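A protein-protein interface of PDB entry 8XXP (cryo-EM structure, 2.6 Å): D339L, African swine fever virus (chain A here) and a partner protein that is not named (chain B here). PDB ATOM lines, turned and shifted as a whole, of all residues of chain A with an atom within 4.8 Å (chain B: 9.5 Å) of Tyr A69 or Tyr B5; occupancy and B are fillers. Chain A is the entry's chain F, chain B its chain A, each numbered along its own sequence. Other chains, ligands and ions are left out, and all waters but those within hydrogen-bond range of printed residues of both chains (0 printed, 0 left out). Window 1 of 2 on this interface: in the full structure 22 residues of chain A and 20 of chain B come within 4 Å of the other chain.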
ATOM      1  N   THR A  10     -24.581  32.622  23.212  1.00  0.00           N
ATOM      2  CA  THR A  10     -24.732  31.189  23.404  1.00  0.00           C
ATOM      3  C   THR A  10     -23.356  30.558  23.289  1.00  0.00           C
ATOM      4  O   THR A  10     -22.700  30.685  22.251  1.00  0.00           O
ATOM      5  CB  THR A  10     -25.689  30.579  22.386  1.00  0.00           C
ATOM      6  OG1 THR A  10     -27.000  31.107  22.590  1.00  0.00           O
ATOM      7  CG2 THR A  10     -25.739  29.086  22.549  1.00  0.00           C
ATOM      8  N   LEU A  11     -22.913  29.904  24.354  1.00  0.00           N
ATOM      9  CA  LEU A  11     -21.655  29.182  24.316  1.00  0.00           C
ATOM     10  C   LEU A  11     -21.864  27.815  23.677  1.00  0.00           C
ATOM     11  O   LEU A  11     -22.977  27.428  23.325  1.00  0.00           O
ATOM     12  CB  LEU A  11     -21.066  29.060  25.716  1.00  0.00           C
ATOM     13  CG  LEU A  11     -20.510  30.364  26.287  1.00  0.00           C
ATOM     14  CD1 LEU A  11     -19.744  30.107  27.564  1.00  0.00           C
ATOM     15  CD2 LEU A  11     -19.627  31.055  25.270  1.00  0.00           C
ATOM     16  N   ASN A  12     -20.774  27.090  23.482  1.00  0.00           N
ATOM     17  CA  ASN A  12     -20.819  25.717  23.011  1.00  0.00           C
ATOM     18  C   ASN A  12     -19.996  24.886  23.974  1.00  0.00           C
ATOM     19  O   ASN A  12     -18.859  25.243  24.291  1.00  0.00           O
ATOM     20  CB  ASN A  12     -20.279  25.586  21.587  1.00  0.00           C
ATOM     21  CG  ASN A  12     -21.300  25.957  20.543  1.00  0.00           C
ATOM     22  OD1 ASN A  12     -22.070  26.891  20.724  1.00  0.00           O
ATOM     23  ND2 ASN A  12     -21.307  25.233  19.438  1.00  0.00           N
ATOM     24  N   ILE A  13     -20.569  23.789  24.438  1.00  0.00           N
ATOM     25  CA  ILE A  13     -19.989  23.000  25.510  1.00  0.00           C
ATOM     26  C   ILE A  13     -19.654  21.629  24.939  1.00  0.00           C
ATOM     27  O   ILE A  13     -20.530  20.776  24.777  1.00  0.00           O
ATOM     28  CB  ILE A  13     -20.933  22.911  26.708  1.00  0.00           C
ATOM     29  CG1 ILE A  13     -21.287  24.323  27.168  1.00  0.00           C
ATOM     30  CG2 ILE A  13     -20.289  22.144  27.817  1.00  0.00           C
ATOM     31  CD1 ILE A  13     -22.506  24.400  28.007  1.00  0.00           C
ATOM     32  N   PHE A  58     -28.403  22.972  27.920  1.00  0.00           N
ATOM     33  CA  PHE A  58     -29.172  22.229  26.939  1.00  0.00           C
ATOM     34  C   PHE A  58     -28.239  21.365  26.110  1.00  0.00           C
ATOM     35  O   PHE A  58     -27.116  21.760  25.813  1.00  0.00           O
ATOM     36  CB  PHE A  58     -29.933  23.180  26.019  1.00  0.00           C
ATOM     37  CG  PHE A  58     -30.797  24.173  26.732  1.00  0.00           C
ATOM     38  CD1 PHE A  58     -31.941  23.771  27.381  1.00  0.00           C
ATOM     39  CD2 PHE A  58     -30.480  25.513  26.719  1.00  0.00           C
ATOM     40  CE1 PHE A  58     -32.738  24.683  28.027  1.00  0.00           C
ATOM     41  CE2 PHE A  58     -31.281  26.428  27.357  1.00  0.00           C
ATOM     42  CZ  PHE A  58     -32.411  26.010  28.013  1.00  0.00           C
ATOM     43  N   ILE A  59     -28.703  20.183  25.739  1.00  0.00           N
ATOM     44  CA  ILE A  59     -27.961  19.311  24.838  1.00  0.00           C
ATOM     45  C   ILE A  59     -28.367  19.653  23.416  1.00  0.00           C
ATOM     46  O   ILE A  59     -29.555  19.839  23.134  1.00  0.00           O
ATOM     47  CB  ILE A  59     -28.230  17.832  25.156  1.00  0.00           C
ATOM     48  CG1 ILE A  59     -27.745  17.497  26.564  1.00  0.00           C
ATOM     49  CG2 ILE A  59     -27.551  16.931  24.143  1.00  0.00           C
ATOM     50  CD1 ILE A  59     -26.349  17.947  26.835  1.00  0.00           C
ATOM     51  N   MET A  60     -27.385  19.764  22.523  1.00  0.00           N
ATOM     52  CA  MET A  60     -27.679  20.076  21.132  1.00  0.00           C
ATOM     53  C   MET A  60     -28.613  19.031  20.552  1.00  0.00           C
ATOM     54  O   MET A  60     -28.417  17.830  20.740  1.00  0.00           O
ATOM     55  CB  MET A  60     -26.397  20.145  20.310  1.00  0.00           C
ATOM     56  CG  MET A  60     -25.403  21.153  20.820  1.00  0.00           C
ATOM     57  SD  MET A  60     -23.911  21.221  19.833  1.00  0.00           S
ATOM     58  CE  MET A  60     -23.214  22.743  20.439  1.00  0.00           C
ATOM     59  N   ARG A  61     -29.639  19.496  19.851  1.00  0.00           N
ATOM     60  CA  ARG A  61     -30.688  18.625  19.349  1.00  0.00           C
ATOM     61  C   ARG A  61     -30.500  18.234  17.895  1.00  0.00           C
ATOM     62  O   ARG A  61     -30.848  17.114  17.521  1.00  0.00           O
ATOM     63  CB  ARG A  61     -32.047  19.307  19.518  1.00  0.00           C
ATOM     64  CG  ARG A  61     -33.228  18.411  19.297  1.00  0.00           C
ATOM     65  CD  ARG A  61     -34.513  19.204  19.323  1.00  0.00           C
ATOM     66  NE  ARG A  61     -34.572  20.187  18.249  1.00  0.00           N
ATOM     67  CZ  ARG A  61     -34.875  19.908  16.990  1.00  0.00           C
ATOM     68  NH1 ARG A  61     -35.134  18.674  16.598  1.00  0.00           N
ATOM     69  NH2 ARG A  61     -34.921  20.895  16.100  1.00  0.00           N
ATOM     70  N   THR A  62     -29.942  19.111  17.074  1.00  0.00           N
ATOM     71  CA  THR A  62     -29.915  18.894  15.637  1.00  0.00           C
ATOM     72  C   THR A  62     -28.687  18.133  15.162  1.00  0.00           C
ATOM     73  O   THR A  62     -28.554  17.905  13.958  1.00  0.00           O
ATOM     74  CB  THR A  62     -30.012  20.232  14.905  1.00  0.00           C
ATOM     75  OG1 THR A  62     -29.087  21.158  15.481  1.00  0.00           O
ATOM     76  CG2 THR A  62     -31.415  20.790  15.023  1.00  0.00           C
ATOM     77  N   ASN A  63     -27.794  17.734  16.061  1.00  0.00           N
ATOM     78  CA  ASN A  63     -26.662  16.906  15.681  1.00  0.00           C
ATOM     79  C   ASN A  63     -26.450  15.824  16.727  1.00  0.00           C
ATOM     80  O   ASN A  63     -26.847  15.968  17.884  1.00  0.00           O
ATOM     81  CB  ASN A  63     -25.382  17.732  15.493  1.00  0.00           C
ATOM     82  CG  ASN A  63     -25.081  18.623  16.668  1.00  0.00           C
ATOM     83  OD1 ASN A  63     -24.776  18.151  17.758  1.00  0.00           O
ATOM     84  ND2 ASN A  63     -25.155  19.926  16.450  1.00  0.00           N
ATOM     85  N   ARG A  67     -23.139  17.362  22.361  1.00  0.00           N
ATOM     86  CA  ARG A  67     -22.637  18.574  22.982  1.00  0.00           C
ATOM     87  C   ARG A  67     -23.785  19.421  23.521  1.00  0.00           C
ATOM     88  O   ARG A  67     -24.960  19.186  23.236  1.00  0.00           O
ATOM     89  CB  ARG A  67     -21.803  19.376  21.989  1.00  0.00           C
ATOM     90  CG  ARG A  67     -20.473  18.750  21.658  1.00  0.00           C
ATOM     91  CD  ARG A  67     -20.066  19.037  20.233  1.00  0.00           C
ATOM     92  NE  ARG A  67     -19.866  20.457  19.974  1.00  0.00           N
ATOM     93  CZ  ARG A  67     -20.141  21.050  18.819  1.00  0.00           C
ATOM     94  NH1 ARG A  67     -20.663  20.380  17.806  1.00  0.00           N
ATOM     95  NH2 ARG A  67     -19.884  22.346  18.679  1.00  0.00           N
ATOM     96  N   GLY A  68     -23.428  20.419  24.319  1.00  0.00           N
ATOM     97  CA  GLY A  68     -24.402  21.330  24.876  1.00  0.00           C
ATOM     98  C   GLY A  68     -24.083  22.760  24.519  1.00  0.00           C
ATOM     99  O   GLY A  68     -22.980  23.023  24.041  1.00  0.00           O
ATOM    100  N   TYR A  69     -25.010  23.699  24.703  1.00  0.00           N
ATOM    101  CA  TYR A  69     -24.700  25.076  24.342  1.00  0.00           C
ATOM    102  C   TYR A  69     -24.738  26.054  25.510  1.00  0.00           C
ATOM    103  O   TYR A  69     -23.726  26.716  25.752  1.00  0.00           O
ATOM    104  CB  TYR A  69     -25.576  25.560  23.176  1.00  0.00           C
ATOM    105  CG  TYR A  69     -27.028  25.150  23.129  1.00  0.00           C
ATOM    106  CD1 TYR A  69     -27.393  23.849  22.830  1.00  0.00           C
ATOM    107  CD2 TYR A  69     -28.035  26.086  23.301  1.00  0.00           C
ATOM    108  CE1 TYR A  69     -28.710  23.486  22.754  1.00  0.00           C
ATOM    109  CE2 TYR A  69     -29.349  25.727  23.227  1.00  0.00           C
ATOM    110  CZ  TYR A  69     -29.684  24.429  22.951  1.00  0.00           C
ATOM    111  OH  TYR A  69     -31.001  24.063  22.875  1.00  0.00           O
ATOM    112  N   MET A  70     -25.845  26.174  26.242  1.00  0.00           N
ATOM    113  CA  MET A  70     -25.998  27.207  27.273  1.00  0.00           C
ATOM    114  C   MET A  70     -26.028  28.622  26.702  1.00  0.00           C
ATOM    115  O   MET A  70     -25.146  29.011  25.937  1.00  0.00           O
ATOM    116  CB  MET A  70     -24.886  27.144  28.329  1.00  0.00           C
ATOM    117  CG  MET A  70     -25.178  27.980  29.564  1.00  0.00           C
ATOM    118  SD  MET A  70     -24.353  27.446  31.063  1.00  0.00           S
ATOM    119  CE  MET A  70     -24.464  25.680  30.902  1.00  0.00           C
ATOM    120  N   HIS A  71     -27.022  29.409  27.101  1.00  0.00           N
ATOM    121  CA  HIS A  71     -27.090  30.827  26.785  1.00  0.00           C
ATOM    122  C   HIS A  71     -26.626  31.622  27.990  1.00  0.00           C
ATOM    123  O   HIS A  71     -26.889  31.240  29.131  1.00  0.00           O
ATOM    124  CB  HIS A  71     -28.510  31.252  26.417  1.00  0.00           C
ATOM    125  CG  HIS A  71     -29.186  30.340  25.447  1.00  0.00           C
ATOM    126  ND1 HIS A  71     -28.675  30.072  24.198  1.00  0.00           N
ATOM    127  CD2 HIS A  71     -30.334  29.633  25.543  1.00  0.00           C
ATOM    128  CE1 HIS A  71     -29.481  29.242  23.564  1.00  0.00           C
ATOM    129  NE2 HIS A  71     -30.496  28.961  24.359  1.00  0.00           N
ATOM    130  N   GLU B   2     -16.515  32.589  18.579  1.00  0.00           N
ATOM    131  CA  GLU B   2     -17.295  31.361  18.526  1.00  0.00           C
ATOM    132  C   GLU B   2     -18.723  31.664  18.099  1.00  0.00           C
ATOM    133  O   GLU B   2     -19.345  32.598  18.613  1.00  0.00           O
ATOM    134  CB  GLU B   2     -17.286  30.663  19.887  1.00  0.00           C
ATOM    135  CG  GLU B   2     -18.408  29.661  20.094  1.00  0.00           C
ATOM    136  CD  GLU B   2     -18.836  29.559  21.545  1.00  0.00           C
ATOM    137  OE1 GLU B   2     -19.611  30.428  21.990  1.00  0.00           O
ATOM    138  OE2 GLU B   2     -18.398  28.617  22.240  1.00  0.00           O
ATOM    139  N   ALA B   3     -19.237  30.874  17.161  1.00  0.00           N
ATOM    140  CA  ALA B   3     -20.629  30.957  16.744  1.00  0.00           C
ATOM    141  C   ALA B   3     -21.438  29.937  17.533  1.00  0.00           C
ATOM    142  O   ALA B   3     -21.236  28.729  17.383  1.00  0.00           O
ATOM    143  CB  ALA B   3     -20.761  30.710  15.243  1.00  0.00           C
ATOM    144  N   GLY B   4     -22.348  30.423  18.374  1.00  0.00           N
ATOM    145  CA  GLY B   4     -23.070  29.547  19.265  1.00  0.00           C
ATOM    146  C   GLY B   4     -24.145  28.743  18.568  1.00  0.00           C
ATOM    147  O   GLY B   4     -24.583  29.058  17.466  1.00  0.00           O
ATOM    148  N   TYR B   5     -24.575  27.682  19.239  1.00  0.00           N
ATOM    149  CA  TYR B   5     -25.607  26.816  18.692  1.00  0.00           C
ATOM    150  C   TYR B   5     -26.926  27.566  18.582  1.00  0.00           C
ATOM    151  O   TYR B   5     -27.363  28.224  19.527  1.00  0.00           O
ATOM    152  CB  TYR B   5     -25.775  25.579  19.567  1.00  0.00           C
ATOM    153  CG  TYR B   5     -26.819  24.610  19.075  1.00  0.00           C
ATOM    154  CD1 TYR B   5     -26.502  23.636  18.147  1.00  0.00           C
ATOM    155  CD2 TYR B   5     -28.119  24.664  19.543  1.00  0.00           C
ATOM    156  CE1 TYR B   5     -27.446  22.751  17.701  1.00  0.00           C
ATOM    157  CE2 TYR B   5     -29.066  23.782  19.105  1.00  0.00           C
ATOM    158  CZ  TYR B   5     -28.725  22.828  18.185  1.00  0.00           C
ATOM    159  OH  TYR B   5     -29.676  21.947  17.742  1.00  0.00           O
ATOM    160  N   ALA B   6     -27.570  27.451  17.425  1.00  0.00           N
ATOM    161  CA  ALA B   6     -28.843  28.106  17.190  1.00  0.00           C
ATOM    162  C   ALA B   6     -29.716  27.188  16.354  1.00  0.00           C
ATOM    163  O   ALA B   6     -29.226  26.303  15.652  1.00  0.00           O
ATOM    164  CB  ALA B   6     -28.663  29.457  16.494  1.00  0.00           C
ATOM    165  N   GLU B   7     -31.022  27.403  16.449  1.00  0.00           N
ATOM    166  CA  GLU B   7     -31.996  26.684  15.646  1.00  0.00           C
ATOM    167  C   GLU B   7     -32.931  27.682  14.989  1.00  0.00           C
ATOM    168  O   GLU B   7     -33.278  28.701  15.585  1.00  0.00           O
ATOM    169  CB  GLU B   7     -32.804  25.692  16.485  1.00  0.00           C
ATOM    170  CG  GLU B   7     -31.987  24.565  17.074  1.00  0.00           C
ATOM    171  CD  GLU B   7     -32.844  23.485  17.697  1.00  0.00           C
ATOM    172  OE1 GLU B   7     -33.718  22.944  16.994  1.00  0.00           O
ATOM    173  OE2 GLU B   7     -32.643  23.169  18.885  1.00  0.00           O
ATOM    174  N   ILE B   8     -33.340  27.386  13.763  1.00  0.00           N
ATOM    175  CA  ILE B   8     -34.285  28.238  13.053  1.00  0.00           C
ATOM    176  C   ILE B   8     -35.676  27.997  13.622  1.00  0.00           C
ATOM    177  O   ILE B   8     -36.194  26.879  13.568  1.00  0.00           O
ATOM    178  CB  ILE B   8     -34.245  27.969  11.544  1.00  0.00           C
ATOM    179  CG1 ILE B   8     -32.843  28.240  11.006  1.00  0.00           C
ATOM    180  CG2 ILE B   8     -35.257  28.822  10.829  1.00  0.00           C
ATOM    181  CD1 ILE B   8     -32.701  27.999   9.539  1.00  0.00           C
ATOM    182  N   SER B1418     -32.971  21.175   8.828  1.00  0.00           N
ATOM    183  CA  SER B1418     -32.979  20.786  10.222  1.00  0.00           C
ATOM    184  C   SER B1418     -33.671  19.437  10.379  1.00  0.00           C
ATOM    185  O   SER B1418     -33.994  18.758   9.403  1.00  0.00           O
ATOM    186  CB  SER B1418     -33.654  21.867  11.059  1.00  0.00           C
ATOM    187  OG  SER B1418     -33.493  21.603  12.436  1.00  0.00           O
ATOM    188  N   VAL B1419     -33.898  19.042  11.625  1.00  0.00           N
ATOM    189  CA  VAL B1419     -34.538  17.770  11.942  1.00  0.00           C
ATOM    190  C   VAL B1419     -35.861  18.066  12.640  1.00  0.00           C
ATOM    191  O   VAL B1419     -35.922  18.968  13.484  1.00  0.00           O
ATOM    192  CB  VAL B1419     -33.609  16.884  12.789  1.00  0.00           C
ATOM    193  CG1 VAL B1419     -33.199  17.594  14.062  1.00  0.00           C
ATOM    194  CG2 VAL B1419     -34.259  15.554  13.104  1.00  0.00           C
ATOM    195  N   ARG B1421     -38.812  18.225  15.232  1.00  0.00           N
ATOM    196  CA  ARG B1421     -38.836  18.130  16.690  1.00  0.00           C
ATOM    197  C   ARG B1421     -39.942  17.168  17.117  1.00  0.00           C
ATOM    198  O   ARG B1421     -40.956  17.540  17.703  1.00  0.00           O
ATOM    199  CB  ARG B1421     -39.020  19.507  17.307  1.00  0.00           C
ATOM    200  CG  ARG B1421     -38.089  19.804  18.449  1.00  0.00           C
ATOM    201  CD  ARG B1421     -38.697  20.818  19.391  1.00  0.00           C
ATOM    202  NE  ARG B1421     -39.722  20.232  20.245  1.00  0.00           N
ATOM    203  CZ  ARG B1421     -40.995  20.598  20.246  1.00  0.00           C
ATOM    204  NH1 ARG B1421     -41.447  21.533  19.427  1.00  0.00           N
ATOM    205  NH2 ARG B1421     -41.837  20.014  21.094  1.00  0.00           N
ATOM    206  N   MET B1425     -36.525  13.827  19.538  1.00  0.00           N
ATOM    207  CA  MET B1425     -36.199  15.237  19.684  1.00  0.00           C
ATOM    208  C   MET B1425     -37.321  16.044  20.307  1.00  0.00           C
ATOM    209  O   MET B1425     -37.198  17.266  20.406  1.00  0.00           O
ATOM    210  CB  MET B1425     -35.841  15.855  18.334  1.00  0.00           C
ATOM    211  CG  MET B1425     -34.973  15.015  17.450  1.00  0.00           C
ATOM    212  SD  MET B1425     -33.207  15.192  17.706  1.00  0.00           S
ATOM    213  CE  MET B1425     -32.925  14.033  19.028  1.00  0.00           C
ATOM    214  N   SER B1427     -38.600  16.117  23.458  1.00  0.00           N
ATOM    215  CA  SER B1427     -38.273  16.643  24.772  1.00  0.00           C
ATOM    216  C   SER B1427     -36.817  17.073  24.797  1.00  0.00           C
ATOM    217  O   SER B1427     -35.947  16.366  24.280  1.00  0.00           O
ATOM    218  CB  SER B1427     -38.531  15.606  25.864  1.00  0.00           C
ATOM    219  OG  SER B1427     -39.898  15.251  25.919  1.00  0.00           O
ATOM    220  N   ASP B1428     -36.559  18.231  25.386  1.00  0.00           N
ATOM    221  CA  ASP B1428     -35.198  18.704  25.551  1.00  0.00           C
ATOM    222  C   ASP B1428     -34.531  18.015  26.730  1.00  0.00           C
ATOM    223  O   ASP B1428     -35.152  17.792  27.770  1.00  0.00           O
ATOM    224  CB  ASP B1428     -35.177  20.216  25.751  1.00  0.00           C
ATOM    225  CG  ASP B1428     -35.088  20.972  24.444  1.00  0.00           C
ATOM    226  OD1 ASP B1428     -33.960  21.315  24.030  1.00  0.00           O
ATOM    227  OD2 ASP B1428     -36.145  21.224  23.828  1.00  0.00           O
ATOM    228  N   ILE B1429     -33.262  17.678  26.558  1.00  0.00           N
ATOM    229  CA  ILE B1429     -32.438  17.120  27.619  1.00  0.00           C
ATOM    230  C   ILE B1429     -31.518  18.222  28.117  1.00  0.00           C
ATOM    231  O   ILE B1429     -30.869  18.903  27.318  1.00  0.00           O
ATOM    232  CB  ILE B1429     -31.626  15.912  27.123  1.00  0.00           C
ATOM    233  CG1 ILE B1429     -32.528  14.900  26.416  1.00  0.00           C
ATOM    234  CG2 ILE B1429     -30.884  15.268  28.273  1.00  0.00           C
ATOM    235  CD1 ILE B1429     -33.709  14.430  27.228  1.00  0.00           C
ATOM    236  N   ILE B1430     -31.478  18.417  29.428  1.00  0.00           N
ATOM    237  CA  ILE B1430     -30.572  19.371  30.047  1.00  0.00           C
ATOM    238  C   ILE B1430     -29.701  18.621  31.039  1.00  0.00           C
ATOM    239  O   ILE B1430     -30.144  17.653  31.663  1.00  0.00           O
ATOM    240  CB  ILE B1430     -31.321  20.532  30.733  1.00  0.00           C
ATOM    241  CG1 ILE B1430     -32.128  20.031  31.922  1.00  0.00           C
ATOM    242  CG2 ILE B1430     -32.225  21.230  29.748  1.00  0.00           C
ATOM    243  CD1 ILE B1430     -32.920  21.099  32.602  1.00  0.00           C
ATOM    244  N   MET B1431     -28.452  19.047  31.158  1.00  0.00           N
ATOM    245  CA  MET B1431     -27.524  18.366  32.041  1.00  0.00           C
ATOM    246  C   MET B1431     -27.903  18.634  33.492  1.00  0.00           C
ATOM    247  O   MET B1431     -28.218  19.765  33.867  1.00  0.00           O
ATOM    248  CB  MET B1431     -26.100  18.839  31.766  1.00  0.00           C
ATOM    249  CG  MET B1431     -25.599  18.515  30.371  1.00  0.00           C
ATOM    250  SD  MET B1431     -25.155  16.808  30.035  1.00  0.00           S
ATOM    251  CE  MET B1431     -24.359  16.345  31.554  1.00  0.00           C
ATOM    252  N   GLU B1433     -26.864  19.566  36.561  1.00  0.00           N
ATOM    253  CA  GLU B1433     -25.716  20.178  37.220  1.00  0.00           C
ATOM    254  C   GLU B1433     -25.662  19.812  38.696  1.00  0.00           C
ATOM    255  O   GLU B1433     -24.585  19.527  39.229  1.00  0.00           O
ATOM    256  CB  GLU B1433     -25.764  21.693  37.049  1.00  0.00           C
ATOM    257  CG  GLU B1433     -25.740  22.154  35.612  1.00  0.00           C
ATOM    258  CD  GLU B1433     -26.579  23.390  35.394  1.00  0.00           C
ATOM    259  OE1 GLU B1433     -26.714  24.189  36.342  1.00  0.00           O
ATOM    260  OE2 GLU B1433     -27.103  23.567  34.275  1.00  0.00           O
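The side-chain hydroxyl of Tyr B5 is in hydrogen-bond range of the side-chain carboxylate of Glu B7, 3.4 Å away. O of Met A70 is in hydrogen-bond range of N of Leu A11 (2.9 Å). O of Leu A11 lies close to O of Tyr A69. The backbone NH of Met A60 is in hydrogen-bond range of the backbone carbonyl oxygen of Arg A67 (2.6 Å). N of Tyr A69 sits at hydrogen-bond distance from O of Phe A58 (3.1 Å). NH2 of Arg A67 lies close to ND2 of Asn A12.
Of the printed residues of chain B, Leu A11 touches Glu B2 (3.3 Å). Of the printed residues of chain B, Met A60 touches Tyr B5 (3.8 Å). Of the printed residues of chain B, Arg A61 touches Tyr B5 (3.2 Å), Glu B7 (2.5 Å), Ser B1418 (3.996 Å), Val B1419 (3.2 Å), Arg B1421 (3.5 Å) and Met B1425 (3.0 Å). No residue of chain B comes within 4 Å of Met A70. Of the printed residues of chain A, Glu B2 touches Thr A10 (3.1 Å), Leu A11 (3.3 Å) and Asn A12 (3.1 Å). Of the printed residues of chain A, Tyr B5 touches Thr A10 (3.5 Å), Asn A12 (3.0 Å), Met A60 (3.8 Å), Arg A61 (3.2 Å), Thr A62 (2.5 Å), Asn A63 (3.8 Å) and Tyr A69 (3.5 Å). Glu B1433 touches none of the printed residues of chain A.
OE2 of Glu B2 is in hydrogen-bond range of N of Asn A12 (3.1 Å). OH of Tyr B5 is in hydrogen-bond range of OG1 of Thr A62 (2.5 Å). N of Arg A61 lies within hydrogen-bond range of OH of Tyr B5, at 3.2 Å. The backbone carbonyl oxygen (O) of Arg A61 lies close to the side-chain sulfur (SD) of Met B1425 (3.0 Å). The backbone carbonyl oxygen (O) of Ile B1429 is in hydrogen-bond range of the backbone NH (N) of Ile A59. O of Thr A10 lies close to OE1 of Glu B2 (3.1 Å). The guanidinium group (NH2) of Arg A61 is in salt-bridge range of the side-chain carboxylate (OE1) of Glu B7 (2.5 Å). The backbone carbonyl oxygen of Val B1419 sits at hydrogen-bond distance from the guanidinium group of Arg A61, at 3.2 Å. The backbone NH of Tyr B5 is in hydrogen-bond range of the side-chain amide oxygen of Asn A12 (3.0 Å).
Hydrophobic or aromatic side chains of chain A that line the printed part of chain B: Leu A11, Phe A58, Ile A59, Met A60 and Tyr A69. Of the 17 printed residues of chain B, 12 touch a printed residue of chain A. Along chain B the printed residues that touch a printed residue of chain A span positions 2 to 1431. Among the printed residues, Asp or Glu carboxylates within 4 Å of a Lys or Arg side-chain nitrogen of the other chain: Arg A61 with Glu B7 (2.5 Å).
OD1 of Asn A12 touches O of Ala B3 (3.9 Å). OD1 of Asn A12 touches CA of Gly B4, at 3.2 Å. CA of Phe A58 touches O of Ile B1429, 3.8 Å away. Ile B1430 touches Phe A58. CD1 of Tyr B5 touches CG of Met A60, 3.8 Å away. OE1 of Glu B7 touches CG2 of Thr A62, 3.7 Å away. Thr A62 touches Ser B1418. Thr A62 touches Val B1419 (CG2 to CG1, 3.8 Å). Tyr B5 touches Asn A63 (CE1 to ND2, 3.8 Å). Tyr A69 touches Tyr B5 (CD1 to CD2, 3.5 Å).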
